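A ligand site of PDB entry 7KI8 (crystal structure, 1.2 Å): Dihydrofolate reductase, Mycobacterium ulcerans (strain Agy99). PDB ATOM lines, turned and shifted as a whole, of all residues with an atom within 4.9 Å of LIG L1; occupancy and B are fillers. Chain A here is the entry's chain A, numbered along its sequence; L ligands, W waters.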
ATOM      1  N   ILE A  15     -22.672  21.939 -22.598  1.00  0.00           N
ATOM      2  CA  ILE A  15     -21.726  22.833 -23.246  1.00  0.00           C
ATOM      3  C   ILE A  15     -20.699  21.970 -23.970  1.00  0.00           C
ATOM      4  O   ILE A  15     -20.192  21.007 -23.373  1.00  0.00           O
ATOM      5  CB  ILE A  15     -21.089  23.812 -22.244  1.00  0.00           C
ATOM      6  CG1 ILE A  15     -20.165  24.808 -22.961  1.00  0.00           C
ATOM      7  CG2 ILE A  15     -20.393  23.079 -21.065  1.00  0.00           C
ATOM      8  CD1 ILE A  15     -19.753  25.996 -22.101  1.00  0.00           C
ATOM      9  N   TRP A  16     -20.469  22.240 -25.255  1.00  0.00           N
ATOM     10  CA  TRP A  16     -19.506  21.492 -26.039  1.00  0.00           C
ATOM     11  C   TRP A  16     -18.949  22.360 -27.144  1.00  0.00           C
ATOM     12  O   TRP A  16     -19.530  23.370 -27.515  1.00  0.00           O
ATOM     13  CB  TRP A  16     -20.101  20.204 -26.628  1.00  0.00           C
ATOM     14  CG  TRP A  16     -21.037  20.322 -27.790  1.00  0.00           C
ATOM     15  CD1 TRP A  16     -20.704  20.383 -29.109  1.00  0.00           C
ATOM     16  CD2 TRP A  16     -22.482  20.250 -27.750  1.00  0.00           C
ATOM     17  NE1 TRP A  16     -21.841  20.384 -29.880  1.00  0.00           N
ATOM     18  CE2 TRP A  16     -22.942  20.310 -29.077  1.00  0.00           C
ATOM     19  CE3 TRP A  16     -23.424  20.151 -26.711  1.00  0.00           C
ATOM     20  CZ2 TRP A  16     -24.294  20.287 -29.398  1.00  0.00           C
ATOM     21  CZ3 TRP A  16     -24.755  20.136 -27.037  1.00  0.00           C
ATOM     22  CH2 TRP A  16     -25.182  20.198 -28.368  1.00  0.00           C
ATOM     23  N   ALA A  17     -17.806  21.929 -27.678  1.00  0.00           N
ATOM     24  CA  ALA A  17     -17.208  22.485 -28.887  1.00  0.00           C
ATOM     25  C   ALA A  17     -17.168  21.405 -29.959  1.00  0.00           C
ATOM     26  O   ALA A  17     -16.868  20.235 -29.670  1.00  0.00           O
ATOM     27  CB  ALA A  17     -15.793  23.006 -28.608  1.00  0.00           C
ATOM     28  N   ILE A  24     -16.656  15.916 -31.983  1.00  0.00           N
ATOM     29  CA  ILE A  24     -16.279  16.474 -30.682  1.00  0.00           C
ATOM     30  C   ILE A  24     -15.043  15.806 -30.091  1.00  0.00           C
ATOM     31  O   ILE A  24     -14.414  16.406 -29.198  1.00  0.00           O
ATOM     32  CB  ILE A  24     -17.441  16.469 -29.672  1.00  0.00           C
ATOM     33  CG1 ILE A  24     -17.863  15.050 -29.268  1.00  0.00           C
ATOM     34  CG2 ILE A  24     -18.592  17.300 -30.194  1.00  0.00           C
ATOM     35  CD1 ILE A  24     -18.735  15.012 -28.019  1.00  0.00           C
ATOM     36  N   GLY A  25     -14.702  14.591 -30.498  1.00  0.00           N
ATOM     37  CA  GLY A  25     -13.624  13.889 -29.840  1.00  0.00           C
ATOM     38  C   GLY A  25     -13.007  12.876 -30.758  1.00  0.00           C
ATOM     39  O   GLY A  25     -13.679  12.303 -31.625  1.00  0.00           O
ATOM     40  N   ARG A  26     -11.706  12.650 -30.571  1.00  0.00           N
ATOM     41  CA  ARG A  26     -10.975  11.676 -31.378  1.00  0.00           C
ATOM     42  C   ARG A  26      -9.748  11.255 -30.599  1.00  0.00           C
ATOM     43  O   ARG A  26      -9.075  12.101 -30.001  1.00  0.00           O
ATOM     44  CB  ARG A  26     -10.578  12.300 -32.717  1.00  0.00           C
ATOM     45  CG  ARG A  26      -9.672  11.439 -33.599  1.00  0.00           C
ATOM     46  CD  ARG A  26      -9.346  12.154 -34.876  1.00  0.00           C
ATOM     47  NE  ARG A  26     -10.528  12.342 -35.691  1.00  0.00           N
ATOM     48  CZ  ARG A  26     -10.566  13.035 -36.816  1.00  0.00           C
ATOM     49  NH1 ARG A  26      -9.484  13.645 -37.279  1.00  0.00           N
ATOM     50  NH2 ARG A  26     -11.705  13.110 -37.491  1.00  0.00           N
ATOM     51  N   GLY A  28      -9.301   9.888 -27.788  1.00  0.00           N
ATOM     52  CA  GLY A  28      -9.292  10.253 -26.388  1.00  0.00           C
ATOM     53  C   GLY A  28      -9.017  11.710 -26.095  1.00  0.00           C
ATOM     54  O   GLY A  28      -8.696  12.054 -24.952  1.00  0.00           O
ATOM     55  N   GLY A  29      -9.113  12.575 -27.097  1.00  0.00           N
ATOM     56  CA  GLY A  29      -8.887  13.984 -26.887  1.00  0.00           C
ATOM     57  C   GLY A  29      -9.766  14.824 -27.786  1.00  0.00           C
ATOM     58  O   GLY A  29     -10.709  14.310 -28.383  1.00  0.00           O
ATOM     59  N   ILE A  30      -9.456  16.098 -27.902  1.00  0.00           N
ATOM     60  CA  ILE A  30     -10.166  17.026 -28.770  1.00  0.00           C
ATOM     61  C   ILE A  30      -9.232  17.375 -29.922  1.00  0.00           C
ATOM     62  O   ILE A  30      -8.114  17.850 -29.689  1.00  0.00           O
ATOM     63  CB  ILE A  30     -10.637  18.275 -28.002  1.00  0.00           C
ATOM     64  CG1 ILE A  30     -11.643  17.885 -26.894  1.00  0.00           C
ATOM     65  CG2 ILE A  30     -11.215  19.292 -28.957  1.00  0.00           C
ATOM     66  CD1 ILE A  30     -12.136  19.045 -26.014  1.00  0.00           C
ATOM     67  N   TRP A  32      -8.486  19.628 -32.017  1.00  0.00           N
ATOM     68  CA  TRP A  32      -8.084  20.983 -32.379  1.00  0.00           C
ATOM     69  C   TRP A  32      -7.727  21.689 -31.084  1.00  0.00           C
ATOM     70  O   TRP A  32      -8.038  21.231 -29.977  1.00  0.00           O
ATOM     71  CB  TRP A  32      -9.192  21.774 -33.100  1.00  0.00           C
ATOM     72  CG  TRP A  32     -10.411  21.915 -32.248  1.00  0.00           C
ATOM     73  CD1 TRP A  32     -10.619  22.841 -31.244  1.00  0.00           C
ATOM     74  CD2 TRP A  32     -11.570  21.078 -32.263  1.00  0.00           C
ATOM     75  NE1 TRP A  32     -11.846  22.624 -30.654  1.00  0.00           N
ATOM     76  CE2 TRP A  32     -12.440  21.542 -31.250  1.00  0.00           C
ATOM     77  CE3 TRP A  32     -11.935  19.966 -33.024  1.00  0.00           C
ATOM     78  CZ2 TRP A  32     -13.654  20.938 -30.999  1.00  0.00           C
ATOM     79  CZ3 TRP A  32     -13.162  19.383 -32.774  1.00  0.00           C
ATOM     80  CH2 TRP A  32     -13.992  19.863 -31.771  1.00  0.00           C
ATOM     81  N   GLY A  53     -18.583  12.525 -18.075  1.00  0.00           N
ATOM     82  CA  GLY A  53     -18.329  11.093 -18.081  1.00  0.00           C
ATOM     83  C   GLY A  53     -16.906  10.775 -17.721  1.00  0.00           C
ATOM     84  O   GLY A  53     -15.990  11.602 -17.814  1.00  0.00           O
ATOM     85  N   ARG A  54     -16.712   9.525 -17.303  1.00  0.00           N
ATOM     86  CA  ARG A  54     -15.401   9.135 -16.786  1.00  0.00           C
ATOM     87  C   ARG A  54     -14.316   9.198 -17.861  1.00  0.00           C
ATOM     88  O   ARG A  54     -13.165   9.528 -17.563  1.00  0.00           O
ATOM     89  CB  ARG A  54     -15.497   7.758 -16.121  1.00  0.00           C
ATOM     90  CG  ARG A  54     -14.304   7.369 -15.223  1.00  0.00           C
ATOM     91  CD  ARG A  54     -13.139   6.724 -15.997  1.00  0.00           C
ATOM     92  NE  ARG A  54     -13.637   5.625 -16.802  1.00  0.00           N
ATOM     93  CZ  ARG A  54     -13.132   5.276 -17.980  1.00  0.00           C
ATOM     94  NH1 ARG A  54     -12.035   5.851 -18.458  1.00  0.00           N
ATOM     95  NH2 ARG A  54     -13.757   4.351 -18.694  1.00  0.00           N
ATOM     96  N   ARG A  55     -14.649   8.892 -19.116  1.00  0.00           N
ATOM     97  CA  ARG A  55     -13.625   8.981 -20.155  1.00  0.00           C
ATOM     98  C   ARG A  55     -13.128  10.413 -20.322  1.00  0.00           C
ATOM     99  O   ARG A  55     -11.915  10.637 -20.480  1.00  0.00           O
ATOM    100  CB  ARG A  55     -14.152   8.422 -21.471  1.00  0.00           C
ATOM    101  CG  ARG A  55     -14.429   6.942 -21.386  1.00  0.00           C
ATOM    102  CD  ARG A  55     -15.055   6.400 -22.652  1.00  0.00           C
ATOM    103  NE  ARG A  55     -14.179   6.541 -23.794  1.00  0.00           N
ATOM    104  CZ  ARG A  55     -14.309   5.841 -24.913  1.00  0.00           C
ATOM    105  NH1 ARG A  55     -15.243   4.912 -25.044  1.00  0.00           N
ATOM    106  NH2 ARG A  55     -13.474   6.062 -25.928  1.00  0.00           N
ATOM    107  N   THR A  56     -14.041  11.386 -20.244  1.00  0.00           N
ATOM    108  CA  THR A  56     -13.643  12.795 -20.307  1.00  0.00           C
ATOM    109  C   THR A  56     -12.761  13.157 -19.112  1.00  0.00           C
ATOM    110  O   THR A  56     -11.741  13.831 -19.274  1.00  0.00           O
ATOM    111  CB  THR A  56     -14.897  13.678 -20.403  1.00  0.00           C
ATOM    112  OG1 THR A  56     -15.540  13.433 -21.662  1.00  0.00           O
ATOM    113  CG2 THR A  56     -14.572  15.161 -20.276  1.00  0.00           C
ATOM    114  N   SER A  59      -9.443  12.012 -19.782  1.00  0.00           N
ATOM    115  CA  SER A  59      -8.853  12.704 -20.921  1.00  0.00           C
ATOM    116  C   SER A  59      -8.255  14.054 -20.570  1.00  0.00           C
ATOM    117  O   SER A  59      -7.469  14.593 -21.361  1.00  0.00           O
ATOM    118  CB  SER A  59      -9.900  12.910 -22.029  1.00  0.00           C
ATOM    119  OG  SER A  59     -10.715  14.044 -21.764  1.00  0.00           O
ATOM    120  N   VAL A  75     -19.399  10.792 -13.692  1.00  0.00           N
ATOM    121  CA  VAL A  75     -20.361   9.714 -13.820  1.00  0.00           C
ATOM    122  C   VAL A  75     -19.611   8.470 -14.270  1.00  0.00           C
ATOM    123  O   VAL A  75     -18.974   8.481 -15.331  1.00  0.00           O
ATOM    124  CB  VAL A  75     -21.447  10.076 -14.849  1.00  0.00           C
ATOM    125  CG1 VAL A  75     -22.478   8.959 -14.956  1.00  0.00           C
ATOM    126  CG2 VAL A  75     -22.083  11.423 -14.476  1.00  0.00           C
ATOM    127  N   THR A  76     -19.703   7.403 -13.488  1.00  0.00           N
ATOM    128  CA  THR A  76     -18.982   6.165 -13.737  1.00  0.00           C
ATOM    129  C   THR A  76     -19.793   5.007 -13.170  1.00  0.00           C
ATOM    130  O   THR A  76     -20.592   5.188 -12.247  1.00  0.00           O
ATOM    131  CB  THR A  76     -17.581   6.210 -13.090  1.00  0.00           C
ATOM    132  OG1 THR A  76     -16.900   4.951 -13.272  1.00  0.00           O
ATOM    133  CG2 THR A  76     -17.650   6.481 -11.593  1.00  0.00           C
ATOM    134  N   ARG A  77     -19.568   3.809 -13.723  1.00  0.00           N
ATOM    135  CA  ARG A  77     -20.110   2.588 -13.143  1.00  0.00           C
ATOM    136  C   ARG A  77     -19.140   1.941 -12.164  1.00  0.00           C
ATOM    137  O   ARG A  77     -19.500   0.967 -11.505  1.00  0.00           O
ATOM    138  CB  ARG A  77     -20.515   1.597 -14.246  1.00  0.00           C
ATOM    139  CG  ARG A  77     -21.583   2.184 -15.160  1.00  0.00           C
ATOM    140  CD  ARG A  77     -21.994   1.227 -16.270  1.00  0.00           C
ATOM    141  NE  ARG A  77     -22.974   1.784 -17.195  1.00  0.00           N
ATOM    142  CZ  ARG A  77     -22.704   2.271 -18.404  1.00  0.00           C
ATOM    143  NH1 ARG A  77     -21.462   2.366 -18.845  1.00  0.00           N
ATOM    144  NH2 ARG A  77     -23.709   2.625 -19.208  1.00  0.00           N
ATOM    145  N   GLN A  78     -17.927   2.459 -12.060  1.00  0.00           N
ATOM    146  CA  GLN A  78     -16.920   1.903 -11.168  1.00  0.00           C
ATOM    147  C   GLN A  78     -17.136   2.376  -9.727  1.00  0.00           C
ATOM    148  O   GLN A  78     -17.834   3.346  -9.473  1.00  0.00           O
ATOM    149  CB  GLN A  78     -15.536   2.324 -11.629  1.00  0.00           C
ATOM    150  CG  GLN A  78     -15.217   1.927 -13.072  1.00  0.00           C
ATOM    151  CD  GLN A  78     -13.789   2.261 -13.446  1.00  0.00           C
ATOM    152  OE1 GLN A  78     -12.854   1.704 -12.860  1.00  0.00           O
ATOM    153  NE2 GLN A  78     -13.607   3.164 -14.396  1.00  0.00           N
ATOM    154  N   GLY A  90     -23.010   7.401  -9.728  1.00  0.00           N
ATOM    155  CA  GLY A  90     -23.315   6.255 -10.565  1.00  0.00           C
ATOM    156  C   GLY A  90     -24.367   6.490 -11.622  1.00  0.00           C
ATOM    157  O   GLY A  90     -24.695   5.566 -12.370  1.00  0.00           O
ATOM    158  N   SER A  91     -24.898   7.704 -11.731  1.00  0.00           N
ATOM    159  CA  SER A  91     -25.934   8.001 -12.702  1.00  0.00           C
ATOM    160  C   SER A  91     -26.003   9.507 -12.867  1.00  0.00           C
ATOM    161  O   SER A  91     -25.545  10.266 -12.013  1.00  0.00           O
ATOM    162  CB  SER A  91     -27.315   7.487 -12.261  1.00  0.00           C
ATOM    163  OG  SER A  91     -27.802   8.210 -11.129  1.00  0.00           O
ATOM    164  N   ILE A 108     -20.455  18.661 -19.329  1.00  0.00           N
ATOM    165  CA  ILE A 108     -19.310  19.092 -20.118  1.00  0.00           C
ATOM    166  C   ILE A 108     -18.728  17.987 -20.982  1.00  0.00           C
ATOM    167  O   ILE A 108     -17.635  18.148 -21.527  1.00  0.00           O
ATOM    168  CB  ILE A 108     -18.234  19.758 -19.240  1.00  0.00           C
ATOM    169  CG1 ILE A 108     -17.531  18.725 -18.351  1.00  0.00           C
ATOM    170  CG2 ILE A 108     -18.845  20.882 -18.401  1.00  0.00           C
ATOM    171  CD1 ILE A 108     -16.211  19.230 -17.771  1.00  0.00           C
ATOM    172  N   GLY A 109     -19.441  16.865 -21.127  1.00  0.00           N
ATOM    173  CA  GLY A 109     -19.069  15.789 -22.046  1.00  0.00           C
ATOM    174  C   GLY A 109     -18.808  14.483 -21.332  1.00  0.00           C
ATOM    175  O   GLY A 109     -18.820  14.414 -20.104  1.00  0.00           O
ATOM    176  N   GLY A 110     -18.524  13.428 -22.107  1.00  0.00           N
ATOM    177  CA  GLY A 110     -18.446  13.436 -23.555  1.00  0.00           C
ATOM    178  C   GLY A 110     -19.748  12.971 -24.199  1.00  0.00           C
ATOM    179  O   GLY A 110     -20.826  13.228 -23.685  1.00  0.00           O
ATOM    180  N   ALA A 111     -19.636  12.304 -25.362  1.00  0.00           N
ATOM    181  CA  ALA A 111     -20.826  11.933 -26.124  1.00  0.00           C
ATOM    182  C   ALA A 111     -21.792  11.073 -25.316  1.00  0.00           C
ATOM    183  O   ALA A 111     -23.015  11.265 -25.398  1.00  0.00           O
ATOM    184  CB  ALA A 111     -20.416  11.221 -27.418  1.00  0.00           C
ATOM    185  N   GLN A 112     -21.290  10.109 -24.558  1.00  0.00           N
ATOM    186  CA  GLN A 112     -22.205   9.264 -23.799  1.00  0.00           C
ATOM    187  C   GLN A 112     -22.957  10.062 -22.750  1.00  0.00           C
ATOM    188  O   GLN A 112     -24.186   9.900 -22.595  1.00  0.00           O
ATOM    189  CB  GLN A 112     -21.445   8.118 -23.147  1.00  0.00           C
ATOM    190  CG  GLN A 112     -20.856   7.165 -24.126  1.00  0.00           C
ATOM    191  CD  GLN A 112     -20.149   6.010 -23.464  1.00  0.00           C
ATOM    192  OE1 GLN A 112     -20.478   5.643 -22.344  1.00  0.00           O
ATOM    193  NE2 GLN A 112     -19.176   5.421 -24.165  1.00  0.00           N
ATOM    194  N   ILE A 113     -22.260  10.928 -22.035  1.00  0.00           N
ATOM    195  CA  ILE A 113     -22.908  11.724 -21.008  1.00  0.00           C
ATOM    196  C   ILE A 113     -23.833  12.783 -21.628  1.00  0.00           C
ATOM    197  O   ILE A 113     -24.914  13.055 -21.079  1.00  0.00           O
ATOM    198  CB  ILE A 113     -21.886  12.244 -19.978  1.00  0.00           C
ATOM    199  CG1 ILE A 113     -21.804  11.286 -18.778  1.00  0.00           C
ATOM    200  CG2 ILE A 113     -22.203  13.612 -19.488  1.00  0.00           C
ATOM    201  CD1 ILE A 113     -21.533   9.822 -19.100  1.00  0.00           C
ATOM    202  N   TYR A 114     -23.480  13.348 -22.794  1.00  0.00           N
ATOM    203  CA  TYR A 114     -24.406  14.257 -23.461  1.00  0.00           C
ATOM    204  C   TYR A 114     -25.699  13.541 -23.818  1.00  0.00           C
ATOM    205  O   TYR A 114     -26.792  14.102 -23.691  1.00  0.00           O
ATOM    206  CB  TYR A 114     -23.819  14.859 -24.741  1.00  0.00           C
ATOM    207  CG  TYR A 114     -22.691  15.849 -24.560  1.00  0.00           C
ATOM    208  CD1 TYR A 114     -22.745  16.825 -23.571  1.00  0.00           C
ATOM    209  CD2 TYR A 114     -21.578  15.803 -25.369  1.00  0.00           C
ATOM    210  CE1 TYR A 114     -21.693  17.726 -23.403  1.00  0.00           C
ATOM    211  CE2 TYR A 114     -20.533  16.689 -25.212  1.00  0.00           C
ATOM    212  CZ  TYR A 114     -20.589  17.643 -24.229  1.00  0.00           C
ATOM    213  OH  TYR A 114     -19.510  18.489 -24.057  1.00  0.00           O
ATOM    214  N   LEU A 116     -27.087  11.049 -22.258  1.00  0.00           N
ATOM    215  CA  LEU A 116     -27.880  10.880 -21.040  1.00  0.00           C
ATOM    216  C   LEU A 116     -28.538  12.191 -20.627  1.00  0.00           C
ATOM    217  O   LEU A 116     -29.666  12.190 -20.113  1.00  0.00           O
ATOM    218  CB  LEU A 116     -26.991  10.397 -19.898  1.00  0.00           C
ATOM    219  CG  LEU A 116     -26.458   8.972 -19.967  1.00  0.00           C
ATOM    220  CD1 LEU A 116     -25.502   8.720 -18.800  1.00  0.00           C
ATOM    221  CD2 LEU A 116     -27.627   7.993 -19.967  1.00  0.00           C
ATOM    222  N   ALA A 140     -16.038  10.622 -31.588  1.00  0.00           N
ATOM    223  CA  ALA A 140     -17.218  11.045 -30.848  1.00  0.00           C
ATOM    224  C   ALA A 140     -17.832  12.231 -31.568  1.00  0.00           C
ATOM    225  O   ALA A 140     -17.131  13.170 -31.944  1.00  0.00           O
ATOM    226  CB  ALA A 140     -16.832  11.466 -29.426  1.00  0.00           C
HETATM  227  P1  LIG L   1     -17.712  10.020 -21.792  1.00  0.00           P
HETATM  228  O1  LIG L   1     -16.825  11.119 -21.369  1.00  0.00           O
HETATM  229  O2  LIG L   1     -19.170  10.321 -22.003  1.00  0.00           O
HETATM  230  O3  LIG L   1     -17.531   8.888 -20.649  1.00  0.00           O
HETATM  231  C1  LIG L   1     -18.100   7.575 -20.820  1.00  0.00           C
HETATM  232  C2  LIG L   1     -18.069   6.903 -19.475  1.00  0.00           C
HETATM  233  O4  LIG L   1     -19.098   7.452 -18.620  1.00  0.00           O
HETATM  234  C3  LIG L   1     -18.336   5.392 -19.511  1.00  0.00           C
HETATM  235  O5  LIG L   1     -17.169   4.697 -19.924  1.00  0.00           O
HETATM  236  C4  LIG L   1     -18.755   5.182 -18.054  1.00  0.00           C
HETATM  237  O6  LIG L   1     -17.644   5.263 -17.131  1.00  0.00           O
HETATM  238  C5  LIG L   1     -19.605   6.420 -17.784  1.00  0.00           C
HETATM  239  N1  LIG L   1     -21.012   6.210 -18.090  1.00  0.00           N
HETATM  240  C6  LIG L   1     -21.647   6.258 -19.300  1.00  0.00           C
HETATM  241  N2  LIG L   1     -22.934   5.998 -19.244  1.00  0.00           N
HETATM  242  C7  LIG L   1     -23.158   5.766 -17.890  1.00  0.00           C
HETATM  243  C8  LIG L   1     -24.321   5.431 -17.164  1.00  0.00           C
HETATM  244  N3  LIG L   1     -25.523   5.258 -17.724  1.00  0.00           N
HETATM  245  N4  LIG L   1     -24.196   5.274 -15.831  1.00  0.00           N
HETATM  246  C9  LIG L   1     -22.993   5.432 -15.270  1.00  0.00           C
HETATM  247  N5  LIG L   1     -21.833   5.738 -15.850  1.00  0.00           N
HETATM  248  C10 LIG L   1     -21.984   5.893 -17.167  1.00  0.00           C
HETATM  249  O7  LIG L   1     -17.093   9.257 -23.036  1.00  0.00           O
HETATM  250  P2  LIG L   1     -17.127   9.444 -24.619  1.00  0.00           P
HETATM  251  O8  LIG L   1     -18.528   9.478 -25.071  1.00  0.00           O
HETATM  252  O9  LIG L   1     -16.212   8.433 -25.170  1.00  0.00           O
HETATM  253  O10 LIG L   1     -16.542  10.909 -24.793  1.00  0.00           O
HETATM  254  C11 LIG L   1     -15.127  11.142 -24.627  1.00  0.00           C
HETATM  255  C12 LIG L   1     -14.609  11.921 -25.819  1.00  0.00           C
HETATM  256  O11 LIG L   1     -15.292  13.198 -25.904  1.00  0.00           O
HETATM  257  C13 LIG L   1     -13.115  12.246 -25.766  1.00  0.00           C
HETATM  258  O12 LIG L   1     -12.593  12.255 -27.088  1.00  0.00           O
HETATM  259  C14 LIG L   1     -13.124  13.683 -25.230  1.00  0.00           C
HETATM  260  O13 LIG L   1     -11.936  14.373 -25.613  1.00  0.00           O
HETATM  261  C15 LIG L   1     -14.322  14.213 -25.976  1.00  0.00           C
HETATM  262  N6  LIG L   1     -14.901  15.458 -25.365  1.00  0.00           N
HETATM  263  C16 LIG L   1     -15.093  16.508 -26.188  1.00  0.00           C
HETATM  264  C17 LIG L   1     -15.668  17.663 -25.707  1.00  0.00           C
HETATM  265  C18 LIG L   1     -15.896  18.865 -26.600  1.00  0.00           C
HETATM  266  O14 LIG L   1     -16.559  19.822 -26.176  1.00  0.00           O
HETATM  267  N7  LIG L   1     -15.389  18.826 -27.835  1.00  0.00           N
HETATM  268  C19 LIG L   1     -16.022  17.722 -24.359  1.00  0.00           C
HETATM  269  C20 LIG L   1     -15.796  16.631 -23.538  1.00  0.00           C
HETATM  270  C21 LIG L   1     -15.224  15.495 -24.061  1.00  0.00           C
HETATM  271  P3  LIG L   1     -16.942   3.918 -16.620  1.00  0.00           P
HETATM  272  O15 LIG L   1     -17.990   3.090 -15.963  1.00  0.00           O
HETATM  273  O16 LIG L   1     -16.382   3.285 -17.895  1.00  0.00           O
HETATM  274  O17 LIG L   1     -15.901   4.415 -15.675  1.00  0.00           O
HETATM  275  C1  LG2 L   2     -10.060  20.138 -22.003  1.00  0.00           C
HETATM  276  C2  LG2 L   2      -9.659  19.197 -22.942  1.00  0.00           C
HETATM  277  C3  LG2 L   2      -8.378  19.240 -23.495  1.00  0.00           C
HETATM  278  C4  LG2 L   2      -7.482  20.211 -23.119  1.00  0.00           C
HETATM  279  C5  LG2 L   2      -7.867  21.166 -22.191  1.00  0.00           C
HETATM  280  C6  LG2 L   2      -9.117  21.153 -21.626  1.00  0.00           C
HETATM  281  C7  LG2 L   2     -10.932  24.093 -20.089  1.00  0.00           C
HETATM  282  C8  LG2 L   2     -10.277  23.253 -21.184  1.00  0.00           C
HETATM  283  C9  LG2 L   2     -10.708  25.133 -17.795  1.00  0.00           C
HETATM  284  C10 LG2 L   2     -12.336  23.678 -23.855  1.00  0.00           C
HETATM  285  C11 LG2 L   2     -12.976  22.376 -24.366  1.00  0.00           C
HETATM  286  C12 LG2 L   2     -14.472  22.454 -24.230  1.00  0.00           C
HETATM  287  C13 LG2 L   2     -16.410  23.632 -24.732  1.00  0.00           C
HETATM  288  C14 LG2 L   2     -16.608  21.741 -23.442  1.00  0.00           C
HETATM  289  C15 LG2 L   2     -15.197  21.555 -23.510  1.00  0.00           C
HETATM  290  C16 LG2 L   2     -14.299  20.645 -21.485  1.00  0.00           C
HETATM  291  C17 LG2 L   2     -13.642  19.345 -21.024  1.00  0.00           C
HETATM  292  C18 LG2 L   2     -12.279  19.090 -21.707  1.00  0.00           C
HETATM  293  C19 LG2 L   2      -8.481  22.570 -19.729  1.00  0.00           C
HETATM  294  C20 LG2 L   2      -8.986  23.421 -18.562  1.00  0.00           C
HETATM  295  C21 LG2 L   2      -9.924  24.543 -19.029  1.00  0.00           C
HETATM  296  N1  LG2 L   2     -15.086  23.490 -24.824  1.00  0.00           N
HETATM  297  N2  LG2 L   2     -17.007  24.704 -25.314  1.00  0.00           N
HETATM  298  N3  LG2 L   2     -17.182  22.793 -24.045  1.00  0.00           N
HETATM  299  N4  LG2 L   2     -17.405  20.864 -22.779  1.00  0.00           N
HETATM  300  N5  LG2 L   2     -11.319  20.139 -21.433  1.00  0.00           N
HETATM  301  N6  LG2 L   2      -9.554  22.107 -20.666  1.00  0.00           N
HETATM  302  O1  LG2 L   2     -14.652  20.467 -22.878  1.00  0.00           O
HETATM  303  O2  LG2 L   2     -10.048  25.406 -16.773  1.00  0.00           O
HETATM  304  O3  LG2 L   2     -11.927  25.286 -17.968  1.00  0.00           O
HETATM  305  O   HOH W   1     -10.992  15.885 -23.690  1.00  0.00           O
HETATM  306  O   HOH W   2     -17.419   0.435 -15.427  1.00  0.00           O
HETATM  307  O   HOH W   3     -26.397   4.367 -14.455  1.00  0.00           O
HETATM  308  O   HOH W   4     -26.484   4.187 -20.335  1.00  0.00           O
HETATM  309  O   HOH W   5     -15.991   8.420 -27.946  1.00  0.00           O
HETATM  310  O   HOH W   6     -14.590   1.079 -17.779  1.00  0.00           O
HETATM  311  O   HOH W   7     -24.465   5.471 -21.416  1.00  0.00           O
HETATM  312  O   HOH W   8     -18.966   7.317 -26.878  1.00  0.00           O
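O12 of LIG L1 is in hydrogen-bond range of N of Gly 29.
O14 of LIG L1 lies within hydrogen-bond range of N of Ala 17, 2.9 Å away.
The backbone carbonyl oxygen (O) of Ile 24 sits at hydrogen-bond distance from a nitrogen (N7) of LIG L1.
N of Ile 113 sits at hydrogen-bond distance from O2 of LIG L1 (3.1 Å).
O of Ile 108 lies within hydrogen-bond range of N4 of LG2 L2 (3.0 Å).
The side-chain hydroxyl of Thr 76 lies within hydrogen-bond range of an oxygen (O17) of LIG L1 (2.7 Å).
O of Ala 17 lies within hydrogen-bond range of N7 of LIG L1, at 2.7 Å.
The backbone NH (N) of Arg 55 lies within hydrogen-bond range of an oxygen (O3) of LIG L1 (3.3 Å).
The guanidinium group of Arg 55 is in salt-bridge range of an oxygen (O9) of LIG L1, 3.1 Å away.
O of Gly 29 lies within hydrogen-bond range of O13 of LIG L1, at 3.0 Å.
OH of Tyr 114 lies within hydrogen-bond range of N4 of LG2 L2 (3.4 Å).
The guanidinium group (NH2) of Arg 77 lies close to a nitrogen (N2) of LIG L1, 3.5 Å away.
NE2 of Gln 78 lies within hydrogen-bond range of O17 of LIG L1.
O4 of LIG L1 lies within hydrogen-bond range of N of Arg 54 (3.4 Å).
An oxygen (O8) of LIG L1 sits at hydrogen-bond distance from the backbone NH of Gln 112 (2.9 Å).
An oxygen (O15) of LIG L1 sits at hydrogen-bond distance from the backbone NH (N) of Arg 77, 2.8 Å away.
An oxygen (O8) of LIG L1 is in hydrogen-bond range of the backbone NH (N) of Ala 111 (3.0 Å).
The guanidinium group (NE) of Arg 54 is in salt-bridge range of an oxygen (O17) of LIG L1, 2.8 Å away.
O1 of LIG L1 sits at hydrogen-bond distance from OG1 of Thr 56 (2.7 Å).
O of Ile 15 lies within hydrogen-bond range of N4 of LG2 L2, 2.9 Å away.
The backbone NH of Gly 110 is in hydrogen-bond range of an oxygen (O1) of LIG L1, 3.0 Å away.
N of Thr 56 sits at hydrogen-bond distance from O1 of LIG L1 (3.0 Å).
N of Arg 54 lies within hydrogen-bond range of O of Val 75, at 3.2 Å.
The backbone NH (N) of Gly 110 sits at hydrogen-bond distance from the side-chain hydroxyl (OG1) of Thr 56 (3.0 Å).
The backbone NH (N) of Gly 53 sits at hydrogen-bond distance from the backbone carbonyl oxygen (O) of Gly 109.
OH of Tyr 114 lies close to N of Gly 109, 3.4 Å away.
O of Ala 140 is in hydrogen-bond range of N of Ile 24 (2.8 Å).
The backbone NH (N) of Ala 140 is in hydrogen-bond range of the backbone carbonyl oxygen (O) of Gly 25.
The backbone carbonyl oxygen (O) of Ile 15 lies within hydrogen-bond range of the side-chain hydroxyl (OH) of Tyr 114 (2.7 Å).
The backbone carbonyl oxygen (O) of Ile 108 lies within hydrogen-bond range of the side-chain hydroxyl (OH) of Tyr 114, 3.2 Å away.
An oxygen (O4) of LIG L1 lies close to the backbone carbonyl oxygen of Val 75.
Residues that only touch LIG L1: Trp 16 (3.4 Å), Gly 25 (3.4 Å), Arg 26 (3.6 Å), Gly 28 (3.8 Å), Ile 30 (3.7 Å), Gly 53 (3.5 Å), Gly 90 (3.4 Å), Ile 108 (3.1 Å), Gly 109 (3.7 Å), Tyr 114 (3.6 Å) and Leu 116 (3.6 Å).
Hydrophobic or aromatic side chains within 4 Å of LIG L1: Trp 16, Ile 24, Ile 30, Val 75, Ala 111, Ile 113 and Leu 116.
25 residues have an atom within 4 Å of LIG L1: Trp 16, Ala 17, Ile 24, Gly 25, Arg 26, Gly 28, Gly 29, Ile 30, Gly 53, Arg 54, Arg 55, Thr 56, Val 75, Thr 76, Arg 77, Gln 78, Gly 90, Ile 108, Gly 109, Gly 110, Ala 111, Gln 112, Ile 113, Tyr 114 and Leu 116.
Water W1 bridges an oxygen (O13) of LIG L1 and the side-chain hydroxyl of Ser 59.
Water W3 bridges a nitrogen (N4) of LIG L1 (2.7 Å) and the backbone carbonyl oxygen (O) of Gly 90 (2.9 Å).
Water W6 lies within hydrogen-bond range of O16 of LIG L1 and NH2 of Arg 54.
Water W8 bridges an oxygen (O8) of LIG L1 (2.9 Å) and the side-chain amide nitrogen (NE2) of Gln 112 (3.3 Å).
Water W4 lies within hydrogen-bond range of a nitrogen (N3) of LIG L1 (3.0 Å) and the guanidinium group of Arg 77 (3.4 Å).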
